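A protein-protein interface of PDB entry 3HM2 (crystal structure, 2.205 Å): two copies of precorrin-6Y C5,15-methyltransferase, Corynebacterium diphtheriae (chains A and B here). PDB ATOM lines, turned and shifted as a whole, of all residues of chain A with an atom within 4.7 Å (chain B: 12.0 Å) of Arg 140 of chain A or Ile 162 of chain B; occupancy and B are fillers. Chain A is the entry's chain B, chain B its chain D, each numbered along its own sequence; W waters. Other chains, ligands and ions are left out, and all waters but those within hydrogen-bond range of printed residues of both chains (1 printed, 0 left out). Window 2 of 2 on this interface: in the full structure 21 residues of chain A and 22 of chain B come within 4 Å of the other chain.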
ATOM      1  N   LEU A 136      26.072 -27.588  -5.665  1.00  0.00           N
ATOM      2  CA  LEU A 136      26.081 -27.798  -4.209  1.00  0.00           C
ATOM      3  C   LEU A 136      24.677 -28.181  -3.695  1.00  0.00           C
ATOM      4  O   LEU A 136      24.526 -28.881  -2.677  1.00  0.00           O
ATOM      5  CB  LEU A 136      26.546 -26.533  -3.449  1.00  0.00           C
ATOM      6  CG  LEU A 136      27.834 -25.711  -3.629  1.00  0.00           C
ATOM      7  CD1 LEU A 136      27.763 -24.500  -2.704  1.00  0.00           C
ATOM      8  CD2 LEU A 136      29.146 -26.507  -3.359  1.00  0.00           C
ATOM      9  N   TRP A 137      23.654 -27.699  -4.396  1.00  0.00           N
ATOM     10  CA  TRP A 137      22.267 -27.932  -3.988  1.00  0.00           C
ATOM     11  C   TRP A 137      21.857 -29.376  -4.228  1.00  0.00           C
ATOM     12  O   TRP A 137      20.885 -29.856  -3.643  1.00  0.00           O
ATOM     13  CB  TRP A 137      21.297 -26.963  -4.696  1.00  0.00           C
ATOM     14  CG  TRP A 137      21.357 -25.576  -4.140  1.00  0.00           C
ATOM     15  CD1 TRP A 137      21.736 -24.442  -4.792  1.00  0.00           C
ATOM     16  CD2 TRP A 137      21.061 -25.182  -2.792  1.00  0.00           C
ATOM     17  NE1 TRP A 137      21.679 -23.360  -3.939  1.00  0.00           N
ATOM     18  CE2 TRP A 137      21.269 -23.797  -2.704  1.00  0.00           C
ATOM     19  CE3 TRP A 137      20.634 -25.870  -1.650  1.00  0.00           C
ATOM     20  CZ2 TRP A 137      21.071 -23.096  -1.521  1.00  0.00           C
ATOM     21  CZ3 TRP A 137      20.435 -25.166  -0.481  1.00  0.00           C
ATOM     22  CH2 TRP A 137      20.655 -23.802  -0.423  1.00  0.00           C
ATOM     23  N   ALA A 138      22.613 -30.051  -5.089  1.00  0.00           N
ATOM     24  CA  ALA A 138      22.291 -31.395  -5.545  1.00  0.00           C
ATOM     25  C   ALA A 138      23.195 -32.414  -4.859  1.00  0.00           C
ATOM     26  O   ALA A 138      22.798 -33.572  -4.622  1.00  0.00           O
ATOM     27  CB  ALA A 138      22.436 -31.483  -7.071  1.00  0.00           C
ATOM     28  N   LEU A 139      24.412 -31.989  -4.537  1.00  0.00           N
ATOM     29  CA  LEU A 139      25.297 -32.773  -3.685  1.00  0.00           C
ATOM     30  C   LEU A 139      24.879 -32.679  -2.222  1.00  0.00           C
ATOM     31  O   LEU A 139      25.204 -33.551  -1.416  1.00  0.00           O
ATOM     32  CB  LEU A 139      26.747 -32.311  -3.847  1.00  0.00           C
ATOM     33  CG  LEU A 139      27.248 -32.146  -5.284  1.00  0.00           C
ATOM     34  CD1 LEU A 139      28.651 -31.558  -5.299  1.00  0.00           C
ATOM     35  CD2 LEU A 139      27.212 -33.475  -6.021  1.00  0.00           C
ATOM     36  N   ARG A 140      24.155 -31.617  -1.886  1.00  0.00           N
ATOM     37  CA  ARG A 140      23.538 -31.495  -0.570  1.00  0.00           C
ATOM     38  C   ARG A 140      22.358 -32.450  -0.422  1.00  0.00           C
ATOM     39  O   ARG A 140      22.079 -32.943   0.671  1.00  0.00           O
ATOM     40  CB  ARG A 140      23.082 -30.055  -0.324  1.00  0.00           C
ATOM     41  CG  ARG A 140      22.194 -29.885   0.898  1.00  0.00           C
ATOM     42  CD  ARG A 140      21.947 -28.417   1.201  1.00  0.00           C
ATOM     43  NE  ARG A 140      20.767 -28.222   2.040  1.00  0.00           N
ATOM     44  CZ  ARG A 140      19.618 -28.867   1.873  1.00  0.00           C
ATOM     45  NH1 ARG A 140      19.488 -29.754   0.896  1.00  0.00           N
ATOM     46  NH2 ARG A 140      18.597 -28.627   2.684  1.00  0.00           N
ATOM     47  N   LYS A 141      21.670 -32.709  -1.530  1.00  0.00           N
ATOM     48  CA  LYS A 141      20.418 -33.457  -1.497  1.00  0.00           C
ATOM     49  C   LYS A 141      20.619 -34.839  -0.887  1.00  0.00           C
ATOM     50  O   LYS A 141      20.065 -35.149   0.169  1.00  0.00           O
ATOM     51  CB  LYS A 141      19.832 -33.583  -2.905  1.00  0.00           C
ATOM     52  CG  LYS A 141      19.196 -32.305  -3.428  1.00  0.00           C
ATOM     53  CD  LYS A 141      18.623 -32.505  -4.822  1.00  0.00           C
ATOM     54  CE  LYS A 141      18.008 -31.222  -5.355  1.00  0.00           C
ATOM     55  NZ  LYS A 141      17.445 -31.402  -6.723  1.00  0.00           N
ATOM     56  N   GLN A 142      21.413 -35.668  -1.557  1.00  0.00           N
ATOM     57  CA  GLN A 142      21.826 -36.950  -1.003  1.00  0.00           C
ATOM     58  C   GLN A 142      22.691 -36.761   0.239  1.00  0.00           C
ATOM     59  O   GLN A 142      22.350 -37.233   1.323  1.00  0.00           O
ATOM     60  CB  GLN A 142      22.582 -37.770  -2.051  1.00  0.00           C
ATOM     61  CG  GLN A 142      23.271 -36.931  -3.114  1.00  0.00           C
ATOM     62  CD  GLN A 142      23.716 -37.753  -4.308  1.00  0.00           C
ATOM     63  OE1 GLN A 142      23.936 -38.960  -4.198  1.00  0.00           O
ATOM     64  NE2 GLN A 142      23.849 -37.103  -5.458  1.00  0.00           N
ATOM     65  N   PHE A 143      23.814 -36.070   0.072  1.00  0.00           N
ATOM     66  CA  PHE A 143      24.983 -36.291   0.913  1.00  0.00           C
ATOM     67  C   PHE A 143      24.801 -35.659   2.289  1.00  0.00           C
ATOM     68  O   PHE A 143      25.652 -35.804   3.167  1.00  0.00           O
ATOM     69  CB  PHE A 143      26.240 -35.735   0.241  1.00  0.00           C
ATOM     70  CG  PHE A 143      26.660 -36.496  -0.984  1.00  0.00           C
ATOM     71  CD1 PHE A 143      26.322 -37.830  -1.137  1.00  0.00           C
ATOM     72  CD2 PHE A 143      27.393 -35.878  -1.982  1.00  0.00           C
ATOM     73  CE1 PHE A 143      26.706 -38.533  -2.263  1.00  0.00           C
ATOM     74  CE2 PHE A 143      27.780 -36.575  -3.112  1.00  0.00           C
ATOM     75  CZ  PHE A 143      27.436 -37.904  -3.251  1.00  0.00           C
ATOM     76  N   GLY A 144      23.687 -34.957   2.470  1.00  0.00           N
ATOM     77  CA  GLY A 144      23.442 -34.216   3.695  1.00  0.00           C
ATOM     78  C   GLY A 144      24.123 -32.868   3.565  1.00  0.00           C
ATOM     79  O   GLY A 144      24.471 -32.448   2.472  1.00  0.00           O
ATOM     80  N   GLY A 145      24.313 -32.167   4.665  1.00  0.00           N
ATOM     81  CA  GLY A 145      25.073 -30.944   4.597  1.00  0.00           C
ATOM     82  C   GLY A 145      24.241 -29.695   4.432  1.00  0.00           C
ATOM     83  O   GLY A 145      23.017 -29.740   4.203  1.00  0.00           O
ATOM     84  N   THR A 146      24.934 -28.567   4.523  1.00  0.00           N
ATOM     85  CA  THR A 146      24.291 -27.300   4.733  1.00  0.00           C
ATOM     86  C   THR A 146      25.009 -26.232   3.969  1.00  0.00           C
ATOM     87  O   THR A 146      26.241 -26.151   4.031  1.00  0.00           O
ATOM     88  CB  THR A 146      24.350 -26.937   6.212  1.00  0.00           C
ATOM     89  OG1 THR A 146      23.272 -27.577   6.909  1.00  0.00           O
ATOM     90  CG2 THR A 146      24.249 -25.441   6.398  1.00  0.00           C
ATOM     91  N   ILE A 147      24.224 -25.401   3.277  1.00  0.00           N
ATOM     92  CA  ILE A 147      24.697 -24.305   2.420  1.00  0.00           C
ATOM     93  C   ILE A 147      24.523 -22.856   3.023  1.00  0.00           C
ATOM     94  O   ILE A 147      23.459 -22.526   3.533  1.00  0.00           O
ATOM     95  CB  ILE A 147      23.988 -24.431   1.079  1.00  0.00           C
ATOM     96  CG1 ILE A 147      24.630 -25.541   0.288  1.00  0.00           C
ATOM     97  CG2 ILE A 147      23.994 -23.087   0.265  1.00  0.00           C
ATOM     98  CD1 ILE A 147      23.748 -25.976  -0.853  1.00  0.00           C
ATOM     99  N   TRP A 173      29.378 -24.896   0.920  1.00  0.00           N
ATOM    100  CA  TRP A 173      28.748 -26.104   1.374  1.00  0.00           C
ATOM    101  C   TRP A 173      29.642 -26.773   2.454  1.00  0.00           C
ATOM    102  O   TRP A 173      30.799 -27.071   2.192  1.00  0.00           O
ATOM    103  CB  TRP A 173      28.493 -26.985   0.150  1.00  0.00           C
ATOM    104  CG  TRP A 173      27.742 -28.218   0.472  1.00  0.00           C
ATOM    105  CD1 TRP A 173      26.687 -28.335   1.334  1.00  0.00           C
ATOM    106  CD2 TRP A 173      27.996 -29.532  -0.039  1.00  0.00           C
ATOM    107  NE1 TRP A 173      26.275 -29.642   1.400  1.00  0.00           N
ATOM    108  CE2 TRP A 173      27.058 -30.401   0.563  1.00  0.00           C
ATOM    109  CE3 TRP A 173      28.942 -30.062  -0.932  1.00  0.00           C
ATOM    110  CZ2 TRP A 173      27.027 -31.782   0.292  1.00  0.00           C
ATOM    111  CZ3 TRP A 173      28.917 -31.431  -1.204  1.00  0.00           C
ATOM    112  CH2 TRP A 173      27.957 -32.275  -0.596  1.00  0.00           C
ATOM    113  N   LEU B   8      25.507 -20.555  14.692  1.00  0.00           N
ATOM    114  CA  LEU B   8      26.251 -20.650  13.437  1.00  0.00           C
ATOM    115  C   LEU B   8      26.744 -19.292  12.958  1.00  0.00           C
ATOM    116  O   LEU B   8      27.941 -19.004  12.931  1.00  0.00           O
ATOM    117  CB  LEU B   8      25.343 -21.236  12.364  1.00  0.00           C
ATOM    118  CG  LEU B   8      26.117 -21.657  11.138  1.00  0.00           C
ATOM    119  CD1 LEU B   8      27.169 -22.657  11.551  1.00  0.00           C
ATOM    120  CD2 LEU B   8      25.135 -22.272  10.215  1.00  0.00           C
ATOM    121  N   SER B 153      23.952 -14.994   4.804  1.00  0.00           N
ATOM    122  CA  SER B 153      22.686 -15.703   4.949  1.00  0.00           C
ATOM    123  C   SER B 153      22.905 -17.209   5.035  1.00  0.00           C
ATOM    124  O   SER B 153      24.013 -17.700   4.817  1.00  0.00           O
ATOM    125  CB  SER B 153      21.752 -15.374   3.783  1.00  0.00           C
ATOM    126  OG  SER B 153      21.878 -14.017   3.396  1.00  0.00           O
ATOM    127  N   HIS B 154      21.841 -17.939   5.355  1.00  0.00           N
ATOM    128  CA  HIS B 154      21.954 -19.356   5.682  1.00  0.00           C
ATOM    129  C   HIS B 154      20.737 -20.134   5.190  1.00  0.00           C
ATOM    130  O   HIS B 154      19.640 -19.587   5.085  1.00  0.00           O
ATOM    131  CB  HIS B 154      22.125 -19.546   7.191  1.00  0.00           C
ATOM    132  CG  HIS B 154      23.153 -18.645   7.800  1.00  0.00           C
ATOM    133  ND1 HIS B 154      24.460 -19.035   7.999  1.00  0.00           N
ATOM    134  CD2 HIS B 154      23.067 -17.372   8.255  1.00  0.00           C
ATOM    135  CE1 HIS B 154      25.135 -18.042   8.550  1.00  0.00           C
ATOM    136  NE2 HIS B 154      24.313 -17.021   8.715  1.00  0.00           N
ATOM    137  N   GLU B 155      20.942 -21.413   4.891  1.00  0.00           N
ATOM    138  CA  GLU B 155      19.847 -22.288   4.488  1.00  0.00           C
ATOM    139  C   GLU B 155      18.872 -22.516   5.638  1.00  0.00           C
ATOM    140  O   GLU B 155      19.273 -22.889   6.741  1.00  0.00           O
ATOM    141  CB  GLU B 155      20.390 -23.629   3.987  1.00  0.00           C
ATOM    142  CG  GLU B 155      20.430 -24.717   5.046  1.00  0.00           C
ATOM    143  CD  GLU B 155      20.476 -26.110   4.449  1.00  0.00           C
ATOM    144  OE1 GLU B 155      19.674 -26.968   4.874  1.00  0.00           O
ATOM    145  OE2 GLU B 155      21.313 -26.347   3.553  1.00  0.00           O
ATOM    146  N   HIS B 156      17.589 -22.289   5.374  1.00  0.00           N
ATOM    147  CA  HIS B 156      16.563 -22.399   6.403  1.00  0.00           C
ATOM    148  C   HIS B 156      15.319 -23.101   5.869  1.00  0.00           C
ATOM    149  O   HIS B 156      14.629 -22.582   4.993  1.00  0.00           O
ATOM    150  CB  HIS B 156      16.196 -21.015   6.943  1.00  0.00           C
ATOM    151  CG  HIS B 156      15.262 -21.051   8.113  1.00  0.00           C
ATOM    152  ND1 HIS B 156      15.679 -20.818   9.406  1.00  0.00           N
ATOM    153  CD2 HIS B 156      13.931 -21.294   8.185  1.00  0.00           C
ATOM    154  CE1 HIS B 156      14.646 -20.915  10.223  1.00  0.00           C
ATOM    155  NE2 HIS B 156      13.573 -21.204   9.508  1.00  0.00           N
ATOM    156  N   THR B 157      15.039 -24.284   6.404  1.00  0.00           N
ATOM    157  CA  THR B 157      14.064 -25.187   5.802  1.00  0.00           C
ATOM    158  C   THR B 157      12.666 -24.938   6.356  1.00  0.00           C
ATOM    159  O   THR B 157      12.467 -24.899   7.571  1.00  0.00           O
ATOM    160  CB  THR B 157      14.442 -26.661   6.032  1.00  0.00           C
ATOM    161  OG1 THR B 157      15.770 -26.898   5.547  1.00  0.00           O
ATOM    162  CG2 THR B 157      13.472 -27.579   5.305  1.00  0.00           C
ATOM    163  N   GLY B 159       9.576 -25.521   6.121  1.00  0.00           N
ATOM    164  CA  GLY B 159       8.647 -26.629   6.009  1.00  0.00           C
ATOM    165  C   GLY B 159       9.060 -27.556   4.888  1.00  0.00           C
ATOM    166  O   GLY B 159      10.087 -28.228   4.978  1.00  0.00           O
ATOM    167  N   SER B 160       8.270 -27.597   3.822  1.00  0.00           N
ATOM    168  CA  SER B 160       8.637 -28.388   2.648  1.00  0.00           C
ATOM    169  C   SER B 160       9.619 -27.613   1.770  1.00  0.00           C
ATOM    170  O   SER B 160       9.981 -28.063   0.675  1.00  0.00           O
ATOM    171  CB  SER B 160       7.400 -28.784   1.831  1.00  0.00           C
ATOM    172  OG  SER B 160       6.959 -27.724   0.992  1.00  0.00           O
ATOM    173  N   PHE B 161      10.042 -26.447   2.260  1.00  0.00           N
ATOM    174  CA  PHE B 161      10.947 -25.581   1.510  1.00  0.00           C
ATOM    175  C   PHE B 161      12.187 -25.163   2.279  1.00  0.00           C
ATOM    176  O   PHE B 161      12.189 -25.113   3.508  1.00  0.00           O
ATOM    177  CB  PHE B 161      10.219 -24.338   0.983  1.00  0.00           C
ATOM    178  CG  PHE B 161       9.475 -24.577  -0.293  1.00  0.00           C
ATOM    179  CD1 PHE B 161       9.726 -25.714  -1.044  1.00  0.00           C
ATOM    180  CD2 PHE B 161       8.545 -23.665  -0.757  1.00  0.00           C
ATOM    181  CE1 PHE B 161       9.050 -25.947  -2.221  1.00  0.00           C
ATOM    182  CE2 PHE B 161       7.871 -23.886  -1.944  1.00  0.00           C
ATOM    183  CZ  PHE B 161       8.123 -25.028  -2.675  1.00  0.00           C
ATOM    184  N   ILE B 162      13.238 -24.889   1.509  1.00  0.00           N
ATOM    185  CA  ILE B 162      14.462 -24.238   1.974  1.00  0.00           C
ATOM    186  C   ILE B 162      14.394 -22.789   1.495  1.00  0.00           C
ATOM    187  O   ILE B 162      13.881 -22.502   0.417  1.00  0.00           O
ATOM    188  CB  ILE B 162      15.778 -24.891   1.376  1.00  0.00           C
ATOM    189  CG1 ILE B 162      15.684 -26.419   1.293  1.00  0.00           C
ATOM    190  CG2 ILE B 162      17.022 -24.448   2.151  1.00  0.00           C
ATOM    191  CD1 ILE B 162      15.502 -27.108   2.635  1.00  0.00           C
ATOM    192  N   THR B 163      14.915 -21.877   2.295  1.00  0.00           N
ATOM    193  CA  THR B 163      15.011 -20.491   1.886  1.00  0.00           C
ATOM    194  C   THR B 163      16.297 -20.018   2.520  1.00  0.00           C
ATOM    195  O   THR B 163      16.862 -20.741   3.317  1.00  0.00           O
ATOM    196  CB  THR B 163      13.815 -19.682   2.408  1.00  0.00           C
ATOM    197  OG1 THR B 163      13.534 -20.085   3.753  1.00  0.00           O
ATOM    198  CG2 THR B 163      12.564 -19.924   1.527  1.00  0.00           C
ATOM    199  N   MET B 164      16.766 -18.822   2.203  1.00  0.00           N
ATOM    200  CA  MET B 164      18.059 -18.395   2.739  1.00  0.00           C
ATOM    201  C   MET B 164      17.977 -17.227   3.718  1.00  0.00           C
ATOM    202  O   MET B 164      18.080 -16.076   3.322  1.00  0.00           O
ATOM    203  CB  MET B 164      18.967 -18.025   1.578  1.00  0.00           C
ATOM    204  CG  MET B 164      19.141 -19.175   0.602  1.00  0.00           C
ATOM    205  SD  MET B 164      20.353 -20.545   1.362  1.00  0.00           S
ATOM    206  CE  MET B 164      21.582 -19.307   2.238  1.00  0.00           C
ATOM    207  N   LYS B 165      17.807 -17.509   5.000  1.00  0.00           N
ATOM    208  CA  LYS B 165      17.618 -16.414   5.958  1.00  0.00           C
ATOM    209  C   LYS B 165      18.799 -15.404   6.043  1.00  0.00           C
ATOM    210  O   LYS B 165      19.906 -15.746   6.501  1.00  0.00           O
ATOM    211  CB  LYS B 165      17.209 -16.947   7.348  1.00  0.00           C
ATOM    212  CG  LYS B 165      16.428 -15.939   8.221  1.00  0.00           C
ATOM    213  CD  LYS B 165      15.553 -16.640   9.271  1.00  0.00           C
ATOM    214  CE  LYS B 165      14.304 -15.808   9.621  1.00  0.00           C
ATOM    215  NZ  LYS B 165      13.289 -16.551  10.450  1.00  0.00           N
ATOM    216  N   PRO B 166      18.558 -14.149   5.600  1.00  0.00           N
ATOM    217  CA  PRO B 166      19.618 -13.141   5.665  1.00  0.00           C
ATOM    218  C   PRO B 166      19.849 -12.741   7.112  1.00  0.00           C
ATOM    219  O   PRO B 166      18.910 -12.314   7.786  1.00  0.00           O
ATOM    220  CB  PRO B 166      19.032 -11.945   4.888  1.00  0.00           C
ATOM    221  CG  PRO B 166      17.771 -12.417   4.264  1.00  0.00           C
ATOM    222  CD  PRO B 166      17.297 -13.575   5.095  1.00  0.00           C
HETATM  223  O   HOH W   1      20.666 -29.711   5.559  1.00  0.00           O
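OE2 of Glu 155 of chain B is in salt-bridge range of NE of Arg 140 of chain A.
N of Glu 155 of chain B lies within hydrogen-bond range of O of Ile 147 of chain A, 3.1 Å away.
O of Gly 145 of chain A sits close to NE of Arg 140 of chain A.
The backbone carbonyl oxygen (O) of His 154 of chain B lies within hydrogen-bond range of the backbone NH (N) of Lys 165 of chain B, at 2.8 Å.
The backbone NH of Glu 155 of chain B lies close to the side-chain sulfur of Met 164 of chain B (3.7 Å).
CH2 of Trp 137 of chain A touches SD of Met 164 of chain B, at 3.7 Å.
Ile 162 of chain B touches Arg 140 of chain A.
Glu 155 of chain B touches Gly 145 of chain A.
Glu 155 of chain B touches Thr 146 of chain A.
C of His 154 of chain B touches O of Ile 147 of chain A, 3.98 Å away.
Ile 147 of chain A touches Met 164 of chain B.
No residue of chain B comes within 4 Å of Leu 136 of chain A.
Of chain B, only Met 164 comes within 4 Å of Trp 137 of chain A.
Printed residues of chain B within 4 Å of Arg 140 of chain A: Glu 155 (2.5 Å) and Ile 162 (3.4 Å).
No residue of chain B comes within 4 Å of Phe 143 of chain A.
Gly 144 of chain A touches none of the printed residues of chain B.
Printed residues of chain B within 4 Å of Thr 146 of chain A: Glu 155 (3.3 Å).
Printed residues of chain B within 4 Å of Ile 147 of chain A: His 154 (3.98 Å), Glu 155 (3.1 Å) and Met 164 (3.9 Å).
Trp 173 of chain A touches none of the printed residues of chain B.
His 156 of chain B touches none of the printed residues of chain A.
Printed residues of chain A within 4 Å of Ile 162 of chain B: Arg 140 (3.4 Å).
Printed residues of chain A within 4 Å of Met 164 of chain B: Trp 137 (3.7 Å) and Ile 147 (3.9 Å).
Printed residues of chain B that touch a printed residue of chain A: His 154, Glu 155, Ile 162 and Met 164.
Hydrophobic or aromatic side chains of chain B within 4 Å of the printed part of chain A: Ile 162 and Met 164.
Of the 13 printed residues of chain A, 5 touch a printed residue of chain B.
Hydrophobic or aromatic side chains of chain A within 4 Å of the printed part of chain B: Trp 137.
Along chain A the printed residues that touch a printed residue of chain B span positions 137 to 147.
No position is printed for both chains.
Of the 8 pairs that touch across the chains among the printed residues, none has its exchanged pair printed and touching as well.
Water W1 bridges O of Gly 145 of chain A (2.7 Å) and OE1 of Glu 155 of chain B (3.0 Å).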
